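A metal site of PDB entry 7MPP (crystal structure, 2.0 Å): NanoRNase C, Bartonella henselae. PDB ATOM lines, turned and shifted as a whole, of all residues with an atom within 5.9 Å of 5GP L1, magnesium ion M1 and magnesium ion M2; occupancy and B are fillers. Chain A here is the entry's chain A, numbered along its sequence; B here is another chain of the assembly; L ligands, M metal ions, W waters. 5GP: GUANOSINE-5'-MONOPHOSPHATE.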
ATOM      1  N   ASP A  26     -28.859 -18.845  -8.292  1.00  0.00           N
ATOM      2  CA  ASP A  26     -27.640 -18.093  -7.993  1.00  0.00           C
ATOM      3  C   ASP A  26     -28.015 -16.620  -7.924  1.00  0.00           C
ATOM      4  O   ASP A  26     -29.116 -16.214  -8.343  1.00  0.00           O
ATOM      5  CB  ASP A  26     -26.558 -18.349  -9.050  1.00  0.00           C
ATOM      6  CG  ASP A  26     -25.220 -17.706  -8.697  1.00  0.00           C
ATOM      7  OD1 ASP A  26     -24.827 -17.750  -7.528  1.00  0.00           O
ATOM      8  OD2 ASP A  26     -24.569 -17.143  -9.603  1.00  0.00           O
ATOM      9  N   THR A  27     -27.119 -15.807  -7.370  1.00  0.00           N
ATOM     10  CA  THR A  27     -27.348 -14.365  -7.277  1.00  0.00           C
ATOM     11  C   THR A  27     -26.076 -13.606  -7.647  1.00  0.00           C
ATOM     12  O   THR A  27     -24.964 -14.119  -7.511  1.00  0.00           O
ATOM     13  CB  THR A  27     -27.804 -13.922  -5.875  1.00  0.00           C
ATOM     14  OG1 THR A  27     -26.763 -14.188  -4.914  1.00  0.00           O
ATOM     15  CG2 THR A  27     -29.056 -14.663  -5.448  1.00  0.00           C
ATOM     16  N   GLU A  28     -26.265 -12.364  -8.089  1.00  0.00           N
ATOM     17  CA  GLU A  28     -25.191 -11.385  -8.179  1.00  0.00           C
ATOM     18  C   GLU A  28     -25.555 -10.171  -7.338  1.00  0.00           C
ATOM     19  O   GLU A  28     -26.725  -9.783  -7.276  1.00  0.00           O
ATOM     20  CB  GLU A  28     -24.928 -10.966  -9.629  1.00  0.00           C
ATOM     21  CG  GLU A  28     -24.826 -12.123 -10.581  1.00  0.00           C
ATOM     22  CD  GLU A  28     -23.605 -12.967 -10.315  1.00  0.00           C
ATOM     23  OE1 GLU A  28     -22.640 -12.456  -9.694  1.00  0.00           O
ATOM     24  OE2 GLU A  28     -23.613 -14.143 -10.735  1.00  0.00           O
ATOM     25  N   THR A  29     -24.552  -9.572  -6.717  1.00  0.00           N
ATOM     26  CA  THR A  29     -24.742  -8.498  -5.751  1.00  0.00           C
ATOM     27  C   THR A  29     -23.634  -7.464  -5.939  1.00  0.00           C
ATOM     28  O   THR A  29     -22.709  -7.655  -6.741  1.00  0.00           O
ATOM     29  CB  THR A  29     -24.649  -9.013  -4.312  1.00  0.00           C
ATOM     30  OG1 THR A  29     -23.313  -9.426  -4.089  1.00  0.00           O
ATOM     31  CG2 THR A  29     -25.600 -10.189  -4.038  1.00  0.00           C
ATOM     32  N   LEU A  30     -23.681  -6.400  -5.142  1.00  0.00           N
ATOM     33  CA  LEU A  30     -22.586  -5.446  -5.109  1.00  0.00           C
ATOM     34  C   LEU A  30     -21.473  -5.869  -4.145  1.00  0.00           C
ATOM     35  O   LEU A  30     -20.555  -5.098  -3.911  1.00  0.00           O
ATOM     36  CB  LEU A  30     -23.091  -4.043  -4.732  1.00  0.00           C
ATOM     37  CG  LEU A  30     -23.756  -3.297  -5.888  1.00  0.00           C
ATOM     38  CD1 LEU A  30     -24.390  -1.989  -5.413  1.00  0.00           C
ATOM     39  CD2 LEU A  30     -22.718  -3.014  -6.980  1.00  0.00           C
ATOM     40  N   GLY A  31     -21.532  -7.069  -3.602  1.00  0.00           N
ATOM     41  CA  GLY A  31     -20.469  -7.546  -2.740  1.00  0.00           C
ATOM     42  C   GLY A  31     -20.977  -8.590  -1.762  1.00  0.00           C
ATOM     43  O   GLY A  31     -22.091  -9.087  -1.873  1.00  0.00           O
ATOM     44  N   LEU A  32     -20.129  -8.891  -0.776  1.00  0.00           N
ATOM     45  CA  LEU A  32     -20.345 -10.044   0.095  1.00  0.00           C
ATOM     46  C   LEU A  32     -21.047  -9.705   1.402  1.00  0.00           C
ATOM     47  O   LEU A  32     -21.239 -10.601   2.224  1.00  0.00           O
ATOM     48  CB  LEU A  32     -19.017 -10.713   0.417  1.00  0.00           C
ATOM     49  CG  LEU A  32     -18.261 -11.205  -0.817  1.00  0.00           C
ATOM     50  CD1 LEU A  32     -16.905 -11.740  -0.421  1.00  0.00           C
ATOM     51  CD2 LEU A  32     -19.066 -12.269  -1.521  1.00  0.00           C
ATOM     52  N   GLN A  43     -30.612 -15.532 -10.670  1.00  0.00           N
ATOM     53  CA  GLN A  43     -30.618 -16.378 -11.849  1.00  0.00           C
ATOM     54  C   GLN A  43     -31.257 -17.710 -11.488  1.00  0.00           C
ATOM     55  O   GLN A  43     -31.067 -18.215 -10.378  1.00  0.00           O
ATOM     56  CB  GLN A  43     -29.210 -16.619 -12.384  1.00  0.00           C
ATOM     57  CG  GLN A  43     -28.423 -15.361 -12.646  1.00  0.00           C
ATOM     58  CD  GLN A  43     -27.506 -14.995 -11.482  1.00  0.00           C
ATOM     59  OE1 GLN A  43     -27.809 -14.097 -10.712  1.00  0.00           O
ATOM     60  NE2 GLN A  43     -26.380 -15.695 -11.377  1.00  0.00           N
ATOM     61  N   HIS A  80     -24.546 -23.250  -5.543  1.00  0.00           N
ATOM     62  CA  HIS A  80     -23.141 -23.474  -5.203  1.00  0.00           C
ATOM     63  C   HIS A  80     -22.750 -22.479  -4.124  1.00  0.00           C
ATOM     64  O   HIS A  80     -22.693 -21.275  -4.385  1.00  0.00           O
ATOM     65  CB  HIS A  80     -22.209 -23.344  -6.403  1.00  0.00           C
ATOM     66  CG  HIS A  80     -20.779 -23.561  -6.025  1.00  0.00           C
ATOM     67  ND1 HIS A  80     -20.231 -24.816  -5.876  1.00  0.00           N
ATOM     68  CD2 HIS A  80     -19.801 -22.681  -5.695  1.00  0.00           C
ATOM     69  CE1 HIS A  80     -18.969 -24.699  -5.492  1.00  0.00           C
ATOM     70  NE2 HIS A  80     -18.687 -23.413  -5.384  1.00  0.00           N
ATOM     71  N   PHE A  81     -22.445 -22.996  -2.939  1.00  0.00           N
ATOM     72  CA  PHE A  81     -22.202 -22.204  -1.728  1.00  0.00           C
ATOM     73  C   PHE A  81     -23.434 -21.357  -1.419  1.00  0.00           C
ATOM     74  O   PHE A  81     -23.389 -20.121  -1.422  1.00  0.00           O
ATOM     75  CB  PHE A  81     -20.943 -21.342  -1.847  1.00  0.00           C
ATOM     76  CG  PHE A  81     -20.459 -20.788  -0.504  1.00  0.00           C
ATOM     77  CD1 PHE A  81     -20.200 -21.638   0.557  1.00  0.00           C
ATOM     78  CD2 PHE A  81     -20.252 -19.417  -0.330  1.00  0.00           C
ATOM     79  CE1 PHE A  81     -19.758 -21.132   1.796  1.00  0.00           C
ATOM     80  CE2 PHE A  81     -19.810 -18.912   0.899  1.00  0.00           C
ATOM     81  CZ  PHE A  81     -19.554 -19.775   1.962  1.00  0.00           C
ATOM     82  N   PHE A  84     -24.172 -18.177   1.101  1.00  0.00           N
ATOM     83  CA  PHE A  84     -24.205 -16.776   0.713  1.00  0.00           C
ATOM     84  C   PHE A  84     -25.556 -16.396   0.121  1.00  0.00           C
ATOM     85  O   PHE A  84     -26.175 -15.422   0.550  1.00  0.00           O
ATOM     86  CB  PHE A  84     -23.093 -16.460  -0.286  1.00  0.00           C
ATOM     87  CG  PHE A  84     -23.208 -15.076  -0.818  1.00  0.00           C
ATOM     88  CD1 PHE A  84     -22.915 -14.006  -0.002  1.00  0.00           C
ATOM     89  CD2 PHE A  84     -23.721 -14.840  -2.081  1.00  0.00           C
ATOM     90  CE1 PHE A  84     -23.069 -12.693  -0.454  1.00  0.00           C
ATOM     91  CE2 PHE A  84     -23.878 -13.542  -2.551  1.00  0.00           C
ATOM     92  CZ  PHE A  84     -23.554 -12.463  -1.728  1.00  0.00           C
ATOM     93  N   ASP A  85     -26.004 -17.135  -0.901  1.00  0.00           N
ATOM     94  CA  ASP A  85     -27.222 -16.757  -1.612  1.00  0.00           C
ATOM     95  C   ASP A  85     -28.423 -16.798  -0.687  1.00  0.00           C
ATOM     96  O   ASP A  85     -29.318 -15.949  -0.772  1.00  0.00           O
ATOM     97  CB  ASP A  85     -27.446 -17.680  -2.800  1.00  0.00           C
ATOM     98  CG  ASP A  85     -26.292 -17.649  -3.761  1.00  0.00           C
ATOM     99  OD1 ASP A  85     -26.119 -16.611  -4.456  1.00  0.00           O
ATOM    100  OD2 ASP A  85     -25.545 -18.644  -3.803  1.00  0.00           O
ATOM    101  N   LYS A 133     -14.640 -16.737 -14.721  1.00  0.00           N
ATOM    102  CA  LYS A 133     -15.003 -15.848 -13.624  1.00  0.00           C
ATOM    103  C   LYS A 133     -14.675 -14.385 -13.910  1.00  0.00           C
ATOM    104  O   LYS A 133     -14.670 -13.568 -12.979  1.00  0.00           O
ATOM    105  CB  LYS A 133     -14.332 -16.288 -12.320  1.00  0.00           C
ATOM    106  CG  LYS A 133     -14.596 -17.746 -11.897  1.00  0.00           C
ATOM    107  CD  LYS A 133     -16.075 -18.173 -12.103  1.00  0.00           C
ATOM    108  CE  LYS A 133     -17.018 -17.649 -11.023  1.00  0.00           C
ATOM    109  NZ  LYS A 133     -18.479 -17.969 -11.282  1.00  0.00           N
ATOM    110  N   GLN A 136     -17.280 -11.830 -12.780  1.00  0.00           N
ATOM    111  CA  GLN A 136     -17.649 -11.850 -11.365  1.00  0.00           C
ATOM    112  C   GLN A 136     -17.473 -10.471 -10.746  1.00  0.00           C
ATOM    113  O   GLN A 136     -18.404  -9.932 -10.131  1.00  0.00           O
ATOM    114  CB  GLN A 136     -16.801 -12.897 -10.642  1.00  0.00           C
ATOM    115  CG  GLN A 136     -17.025 -13.007  -9.146  1.00  0.00           C
ATOM    116  CD  GLN A 136     -16.149 -14.078  -8.522  1.00  0.00           C
ATOM    117  OE1 GLN A 136     -16.636 -15.145  -8.137  1.00  0.00           O
ATOM    118  NE2 GLN A 136     -14.844 -13.817  -8.449  1.00  0.00           N
ATOM    119  N   SER A 137     -16.300  -9.866 -10.913  1.00  0.00           N
ATOM    120  CA  SER A 137     -16.048  -8.527 -10.395  1.00  0.00           C
ATOM    121  C   SER A 137     -16.425  -7.529 -11.485  1.00  0.00           C
ATOM    122  O   SER A 137     -15.616  -7.171 -12.348  1.00  0.00           O
ATOM    123  CB  SER A 137     -14.604  -8.377  -9.946  1.00  0.00           C
ATOM    124  OG  SER A 137     -14.355  -9.218  -8.824  1.00  0.00           O
ATOM    125  N   SER A 138     -17.672  -7.086 -11.444  1.00  0.00           N
ATOM    126  CA  SER A 138     -18.209  -6.129 -12.389  1.00  0.00           C
ATOM    127  C   SER A 138     -19.357  -5.420 -11.708  1.00  0.00           C
ATOM    128  O   SER A 138     -19.816  -5.840 -10.638  1.00  0.00           O
ATOM    129  CB  SER A 138     -18.670  -6.798 -13.690  1.00  0.00           C
ATOM    130  OG  SER A 138     -19.838  -7.580 -13.485  1.00  0.00           O
ATOM    131  N   TRP A 140     -22.601  -5.060 -10.992  1.00  0.00           N
ATOM    132  CA  TRP A 140     -23.836  -5.814 -11.138  1.00  0.00           C
ATOM    133  C   TRP A 140     -25.086  -4.961 -10.940  1.00  0.00           C
ATOM    134  O   TRP A 140     -26.189  -5.428 -11.276  1.00  0.00           O
ATOM    135  CB  TRP A 140     -23.816  -6.993 -10.179  1.00  0.00           C
ATOM    136  CG  TRP A 140     -22.894  -8.068 -10.686  1.00  0.00           C
ATOM    137  CD1 TRP A 140     -21.680  -8.425 -10.169  1.00  0.00           C
ATOM    138  CD2 TRP A 140     -23.107  -8.908 -11.823  1.00  0.00           C
ATOM    139  NE1 TRP A 140     -21.124  -9.439 -10.912  1.00  0.00           N
ATOM    140  CE2 TRP A 140     -21.988  -9.748 -11.934  1.00  0.00           C
ATOM    141  CE3 TRP A 140     -24.146  -9.016 -12.765  1.00  0.00           C
ATOM    142  CZ2 TRP A 140     -21.871 -10.704 -12.939  1.00  0.00           C
ATOM    143  CZ3 TRP A 140     -24.020  -9.966 -13.761  1.00  0.00           C
ATOM    144  CH2 TRP A 140     -22.891 -10.797 -13.843  1.00  0.00           C
ATOM    145  N   TYR A 152     -22.371 -14.785 -18.108  1.00  0.00           N
ATOM    146  CA  TYR A 152     -21.747 -15.262 -16.877  1.00  0.00           C
ATOM    147  C   TYR A 152     -22.796 -15.629 -15.847  1.00  0.00           C
ATOM    148  O   TYR A 152     -22.743 -16.711 -15.242  1.00  0.00           O
ATOM    149  CB  TYR A 152     -20.809 -14.189 -16.323  1.00  0.00           C
ATOM    150  CG  TYR A 152     -20.375 -14.457 -14.901  1.00  0.00           C
ATOM    151  CD1 TYR A 152     -19.275 -15.249 -14.633  1.00  0.00           C
ATOM    152  CD2 TYR A 152     -21.077 -13.912 -13.817  1.00  0.00           C
ATOM    153  CE1 TYR A 152     -18.864 -15.503 -13.322  1.00  0.00           C
ATOM    154  CE2 TYR A 152     -20.679 -14.150 -12.507  1.00  0.00           C
ATOM    155  CZ  TYR A 152     -19.566 -14.948 -12.269  1.00  0.00           C
ATOM    156  OH  TYR A 152     -19.162 -15.196 -10.978  1.00  0.00           O
ATOM    157  N   ALA A 153     -23.747 -14.726 -15.611  1.00  0.00           N
ATOM    158  CA  ALA A 153     -24.779 -14.999 -14.612  1.00  0.00           C
ATOM    159  C   ALA A 153     -25.524 -16.289 -14.933  1.00  0.00           C
ATOM    160  O   ALA A 153     -25.765 -17.118 -14.045  1.00  0.00           O
ATOM    161  CB  ALA A 153     -25.732 -13.803 -14.539  1.00  0.00           C
ATOM    162  N   ASP A 156     -23.624 -19.695 -14.288  1.00  0.00           N
ATOM    163  CA  ASP A 156     -23.530 -20.114 -12.899  1.00  0.00           C
ATOM    164  C   ASP A 156     -24.710 -20.976 -12.463  1.00  0.00           C
ATOM    165  O   ASP A 156     -24.607 -21.617 -11.414  1.00  0.00           O
ATOM    166  CB  ASP A 156     -23.413 -18.893 -11.988  1.00  0.00           C
ATOM    167  CG  ASP A 156     -21.949 -18.474 -11.749  1.00  0.00           C
ATOM    168  OD1 ASP A 156     -21.062 -19.093 -12.373  1.00  0.00           O
ATOM    169  OD2 ASP A 156     -21.697 -17.543 -10.947  1.00  0.00           O
ATOM    170  N   ARG B 111     -16.405  -0.167  -5.363  1.00  0.00           N
ATOM    171  CA  ARG B 111     -16.165  -1.475  -5.965  1.00  0.00           C
ATOM    172  C   ARG B 111     -16.082  -2.541  -4.870  1.00  0.00           C
ATOM    173  O   ARG B 111     -15.075  -3.207  -4.650  1.00  0.00           O
ATOM    174  CB  ARG B 111     -14.920  -1.436  -6.842  1.00  0.00           C
ATOM    175  CG  ARG B 111     -15.139  -0.495  -8.046  1.00  0.00           C
ATOM    176  CD  ARG B 111     -13.885  -0.301  -8.879  1.00  0.00           C
ATOM    177  NE  ARG B 111     -13.446  -1.547  -9.500  1.00  0.00           N
ATOM    178  CZ  ARG B 111     -12.397  -2.258  -9.117  1.00  0.00           C
ATOM    179  NH1 ARG B 111     -11.659  -1.853  -8.087  1.00  0.00           N
ATOM    180  NH2 ARG B 111     -12.092  -3.366  -9.754  1.00  0.00           N
ATOM    181  N   THR B 112     -17.216  -2.673  -4.182  1.00  0.00           N
ATOM    182  CA  THR B 112     -17.332  -3.583  -3.051  1.00  0.00           C
ATOM    183  C   THR B 112     -17.423  -5.037  -3.496  1.00  0.00           C
ATOM    184  O   THR B 112     -17.355  -5.936  -2.659  1.00  0.00           O
ATOM    185  CB  THR B 112     -18.553  -3.181  -2.202  1.00  0.00           C
ATOM    186  OG1 THR B 112     -19.659  -2.892  -3.071  1.00  0.00           O
ATOM    187  CG2 THR B 112     -18.245  -1.907  -1.409  1.00  0.00           C
ATOM    188  N   TYR B 113     -17.577  -5.262  -4.792  1.00  0.00           N
ATOM    189  CA  TYR B 113     -17.649  -6.590  -5.373  1.00  0.00           C
ATOM    190  C   TYR B 113     -16.281  -7.163  -5.719  1.00  0.00           C
ATOM    191  O   TYR B 113     -16.203  -8.164  -6.424  1.00  0.00           O
ATOM    192  CB  TYR B 113     -18.528  -6.545  -6.613  1.00  0.00           C
ATOM    193  CG  TYR B 113     -18.232  -5.378  -7.551  1.00  0.00           C
ATOM    194  CD1 TYR B 113     -17.132  -5.389  -8.403  1.00  0.00           C
ATOM    195  CD2 TYR B 113     -19.087  -4.280  -7.604  1.00  0.00           C
ATOM    196  CE1 TYR B 113     -16.874  -4.316  -9.278  1.00  0.00           C
ATOM    197  CE2 TYR B 113     -18.846  -3.231  -8.465  1.00  0.00           C
ATOM    198  CZ  TYR B 113     -17.740  -3.248  -9.297  1.00  0.00           C
ATOM    199  OH  TYR B 113     -17.518  -2.187 -10.148  1.00  0.00           O
ATOM    200  N   THR B 114     -15.203  -6.512  -5.270  1.00  0.00           N
ATOM    201  CA  THR B 114     -13.857  -6.996  -5.503  1.00  0.00           C
ATOM    202  C   THR B 114     -12.993  -6.568  -4.333  1.00  0.00           C
ATOM    203  O   THR B 114     -13.380  -5.702  -3.534  1.00  0.00           O
ATOM    204  CB  THR B 114     -13.249  -6.463  -6.806  1.00  0.00           C
ATOM    205  OG1 THR B 114     -11.922  -6.992  -6.963  1.00  0.00           O
ATOM    206  CG2 THR B 114     -13.138  -4.922  -6.754  1.00  0.00           C
ATOM    207  N   ASP B 115     -11.819  -7.163  -4.241  1.00  0.00           N
ATOM    208  CA  ASP B 115     -10.820  -6.776  -3.266  1.00  0.00           C
ATOM    209  C   ASP B 115      -9.584  -6.182  -3.929  1.00  0.00           C
ATOM    210  O   ASP B 115      -8.619  -5.837  -3.239  1.00  0.00           O
ATOM    211  CB  ASP B 115     -10.458  -7.993  -2.404  1.00  0.00           C
ATOM    212  CG  ASP B 115     -11.683  -8.842  -2.057  1.00  0.00           C
ATOM    213  OD1 ASP B 115     -12.693  -8.269  -1.582  1.00  0.00           O
ATOM    214  OD2 ASP B 115     -11.665 -10.074  -2.291  1.00  0.00           O
HETATM  215  P   5GP L   1     -20.852 -15.118  -8.001  1.00  0.00           P
HETATM  216  O1P 5GP L   1     -20.872 -14.260  -9.239  1.00  0.00           O
HETATM  217  O2P 5GP L   1     -22.123 -15.920  -7.757  1.00  0.00           O
HETATM  218  O3P 5GP L   1     -19.585 -15.942  -7.932  1.00  0.00           O
HETATM  219  O5' 5GP L   1     -20.679 -14.082  -6.792  1.00  0.00           O
HETATM  220  C5' 5GP L   1     -21.794 -13.403  -6.200  1.00  0.00           C
HETATM  221  C4' 5GP L   1     -21.438 -11.977  -5.829  1.00  0.00           C
HETATM  222  O4' 5GP L   1     -20.418 -11.986  -4.803  1.00  0.00           O
HETATM  223  C3' 5GP L   1     -20.854 -11.146  -6.960  1.00  0.00           C
HETATM  224  O3' 5GP L   1     -21.871 -10.522  -7.729  1.00  0.00           O
HETATM  225  C2' 5GP L   1     -19.912 -10.158  -6.256  1.00  0.00           C
HETATM  226  O2' 5GP L   1     -20.612  -8.997  -5.842  1.00  0.00           O
HETATM  227  C1' 5GP L   1     -19.513 -10.922  -4.991  1.00  0.00           C
HETATM  228  N9  5GP L   1     -18.143 -11.476  -5.047  1.00  0.00           N
HETATM  229  C8  5GP L   1     -17.743 -12.624  -5.636  1.00  0.00           C
HETATM  230  N7  5GP L   1     -16.428 -12.808  -5.395  1.00  0.00           N
HETATM  231  C5  5GP L   1     -15.995 -11.789  -4.613  1.00  0.00           C
HETATM  232  C6  5GP L   1     -14.768 -11.441  -4.040  1.00  0.00           C
HETATM  233  O6  5GP L   1     -13.747 -12.145  -4.200  1.00  0.00           O
HETATM  234  N1  5GP L   1     -14.694 -10.332  -3.296  1.00  0.00           N
HETATM  235  C2  5GP L   1     -15.762  -9.548  -3.091  1.00  0.00           C
HETATM  236  N2  5GP L   1     -15.657  -8.430  -2.339  1.00  0.00           N
HETATM  237  N3  5GP L   1     -16.960  -9.862  -3.629  1.00  0.00           N
HETATM  238  C4  5GP L   1     -17.093 -10.976  -4.389  1.00  0.00           C
HETATM  239  P   5GP L   2     -16.086 -20.690  -5.187  1.00  0.00           P
HETATM  240  O1P 5GP L   2     -14.565 -20.584  -5.121  1.00  0.00           O
HETATM  241  O2P 5GP L   2     -16.705 -20.803  -6.568  1.00  0.00           O
HETATM  242  O3P 5GP L   2     -16.663 -21.711  -4.248  1.00  0.00           O
HETATM  243  O5' 5GP L   2     -16.571 -19.307  -4.578  1.00  0.00           O
HETATM  244  C5' 5GP L   2     -17.945 -19.059  -4.298  1.00  0.00           C
HETATM  245  C4' 5GP L   2     -18.219 -17.585  -4.195  1.00  0.00           C
HETATM  246  O4' 5GP L   2     -17.628 -17.051  -2.968  1.00  0.00           O
HETATM  247  C3' 5GP L   2     -17.649 -16.752  -5.336  1.00  0.00           C
HETATM  248  O3' 5GP L   2     -18.511 -15.649  -5.601  1.00  0.00           O
HETATM  249  C2' 5GP L   2     -16.328 -16.252  -4.745  1.00  0.00           C
HETATM  250  O2' 5GP L   2     -15.778 -15.107  -5.353  1.00  0.00           O
HETATM  251  C1' 5GP L   2     -16.731 -16.001  -3.296  1.00  0.00           C
HETATM  252  N9  5GP L   2     -15.608 -16.054  -2.362  1.00  0.00           N
HETATM  253  C8  5GP L   2     -14.322 -16.140  -2.755  1.00  0.00           C
HETATM  254  N7  5GP L   2     -13.528 -16.179  -1.661  1.00  0.00           N
HETATM  255  C5  5GP L   2     -14.339 -16.100  -0.582  1.00  0.00           C
HETATM  256  C6  5GP L   2     -14.073 -16.099   0.772  1.00  0.00           C
HETATM  257  O6  5GP L   2     -12.896 -16.171   1.190  1.00  0.00           O
HETATM  258  N1  5GP L   2     -15.101 -16.012   1.632  1.00  0.00           N
HETATM  259  C2  5GP L   2     -16.366 -15.940   1.199  1.00  0.00           C
HETATM  260  N2  5GP L   2     -17.356 -15.860   2.128  1.00  0.00           N
HETATM  261  N3  5GP L   2     -16.652 -15.941  -0.124  1.00  0.00           N
HETATM  262  C4  5GP L   2     -15.646 -16.021  -1.023  1.00  0.00           C
HETATM  263 MG    MG M   1     -22.768 -15.963 -10.060  1.00  0.00          MG
HETATM  264 MG    MG M   2     -22.908 -17.437  -6.612  1.00  0.00          MG
HETATM  265  O   HOH W   1     -17.785  -7.455  -0.427  1.00  0.00           O
HETATM  266  O   HOH W   2     -19.223 -18.584  -8.239  1.00  0.00           O
HETATM  267  O   HOH W   3     -21.092 -17.147  -5.314  1.00  0.00           O
HETATM  268  O   HOH W   4     -22.065 -19.028  -7.886  1.00  0.00           O
HETATM  269  O   HOH W   5     -20.199 -15.032  -3.779  1.00  0.00           O
HETATM  270  O   HOH W   6     -23.740 -18.921  -5.386  1.00  0.00           O
HETATM  271  O   HOH W   7     -23.920 -15.827  -5.692  1.00  0.00           O
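The side-chain hydroxyl (OH) of Tyr 152 is in hydrogen-bond range of an oxygen (O1P) of 5GP L1 (2.6 Å). The side-chain amide oxygen of Gln 136 lies close to an oxygen (O3P) of 5GP L1 (3.1 Å). A ring nitrogen (NE2) of His 80 is in hydrogen-bond range of an oxygen (O3P) of 5GP L2 (2.9 Å). An oxygen (O3') of 5GP L1 is in hydrogen-bond range of the backbone NH of Thr 29. A nitrogen (N2) of 5GP L1 lies within hydrogen-bond range of the backbone carbonyl oxygen (O) of Thr 112 of chain B (3.0 Å). OG1 of Thr 29 is in hydrogen-bond range of O2' of 5GP L1 (3.2 Å). The backbone NH (N) of Gly 31 is in hydrogen-bond range of an oxygen (O2') of 5GP L1, at 3.1 Å. An oxygen (O3') of 5GP L1 sits close to the indole nitrogen of Trp 140, 3.4 Å away. The side-chain amide oxygen (OE1) of Gln 136 is in hydrogen-bond range of an oxygen (O2') of 5GP L2 (2.9 Å). N2 of 5GP L1 sits at hydrogen-bond distance from OD1 of Asp 115 of chain B. An oxygen (O2') of 5GP L1 sits at hydrogen-bond distance from the backbone carbonyl oxygen (O) of Thr 29 (2.6 Å).
An oxygen (O3') of 5GP L2 is in hydrogen-bond range of an oxygen (O3P) of 5GP L1, 2.6 Å away.
The side-chain amide nitrogen (NE2) of Gln 43 sits close to the side-chain carboxylate (OE2) of Glu 28. The side-chain hydroxyl (OG1) of Thr 29 lies within hydrogen-bond range of the backbone carbonyl oxygen (O) of Gly 31, 2.6 Å away. The side-chain hydroxyl (OG1) of Thr 112 of chain B sits at hydrogen-bond distance from the backbone carbonyl oxygen (O) of Leu 30 (2.5 Å). The side-chain hydroxyl (OG1) of Thr 27 is in hydrogen-bond range of the side-chain carboxylate (OD1) of Asp 85 (2.5 Å). NZ of Lys 133 lies within salt-bridge range of OD1 of Asp 156, 3.0 Å away. O of Ala 153 lies within hydrogen-bond range of NE2 of Gln 43 (3.1 Å). The backbone carbonyl oxygen (O) of Leu 30 lies within hydrogen-bond range of the backbone NH (N) of Tyr 113 of chain B, at 3.1 Å. NZ of Lys 133 sits at hydrogen-bond distance from OH of Tyr 152.
O of Thr 27 sits close to O2P of 5GP L1 (3.4 Å). A nitrogen (N3) of 5GP L1 sits close to the backbone carbonyl oxygen (O) of Tyr 113 of chain B. C of Leu 30 touches O2' of 5GP L1 (3.7 Å). CG of Leu 32 touches N3 of 5GP L1 (3.4 Å). Thr 114 of chain B touches 5GP L1. Hydrophobic or aromatic side chains within 4 Å of 5GP L1: Leu 32, Trp 140, Tyr 152 and Tyr 113 of chain B. Within 4 Å of 5GP L1: Asp 26, Thr 27, Glu 28, Thr 29, Leu 30, Gly 31, Leu 32, Gln 136, Trp 140, Tyr 152, Asp 156, Thr 112 of chain B, Tyr 113 of chain B, Thr 114 of chain B and Asp 115 of chain B. Along chain A the residues within 4 Å of 5GP L1 span positions 26 to 156.
Merely in contact with magnesium ion M1: Thr 27 (3.8 Å), Gln 43 (3.9 Å) and Tyr 152 (3.7 Å). The nearest printed residue that does not touch magnesium ion M1 is Lys 133 (4.9 Å).
Merely in contact with magnesium ion M2: Asp 85. Along chain A the residues within 4 Å of magnesium ion M2 span positions 26 to 85. The nearest printed residue that does not touch magnesium ion M2 is Thr 27 (4.01 Å).
OD2 of Asp 156 is bound to magnesium ion M1 (2.1 Å). The side-chain carboxylate (OE2) of Glu 28 is bound to magnesium ion M1, at 2.1 Å. Magnesium ion M1 is bound by OD2 of Asp 26 (2.2 Å). Magnesium ion M1 is bound by an oxygen (O2P) of 5GP L1, 2.4 Å away. Slightly farther from magnesium ion M1 lies O1P of 5GP L1 (2.7 Å).
Magnesium ion M2 is bound by an oxygen (O2P) of 5GP L1 (2.1 Å), water W6 (2.1 Å), water W7 (2.1 Å), the side-chain carboxylate (OD1) of Asp 26 (2.1 Å), water W4 (2.2 Å) and water W3 (2.3 Å). Magnesium ion M2 has six donor atoms within binding distance.
Water W6 bridges OD2 of Asp 85 (2.4 Å) and O of His 80 (2.8 Å). Water W3 lies within hydrogen-bond range of O3' of 5GP L2 (3.0 Å) and O3P of 5GP L1 (3.3 Å). Water W7 bridges the side-chain carboxylate (OD1) of Asp 85 and the backbone carbonyl oxygen (O) of Thr 27. Water W2 lies within hydrogen-bond range of O3P of 5GP L1 (2.7 Å) and NZ of Lys 133 (3.2 Å). Water W1 lies within hydrogen-bond range of the backbone carbonyl oxygen (O) of Thr 112 of chain B (2.7 Å), the backbone NH (N) of Leu 32 (2.8 Å) and a nitrogen (N2) of 5GP L1 (3.0 Å). Water W5 bridges O3' of 5GP L2 (2.6 Å) and O5' of 5GP L1 (3.2 Å).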
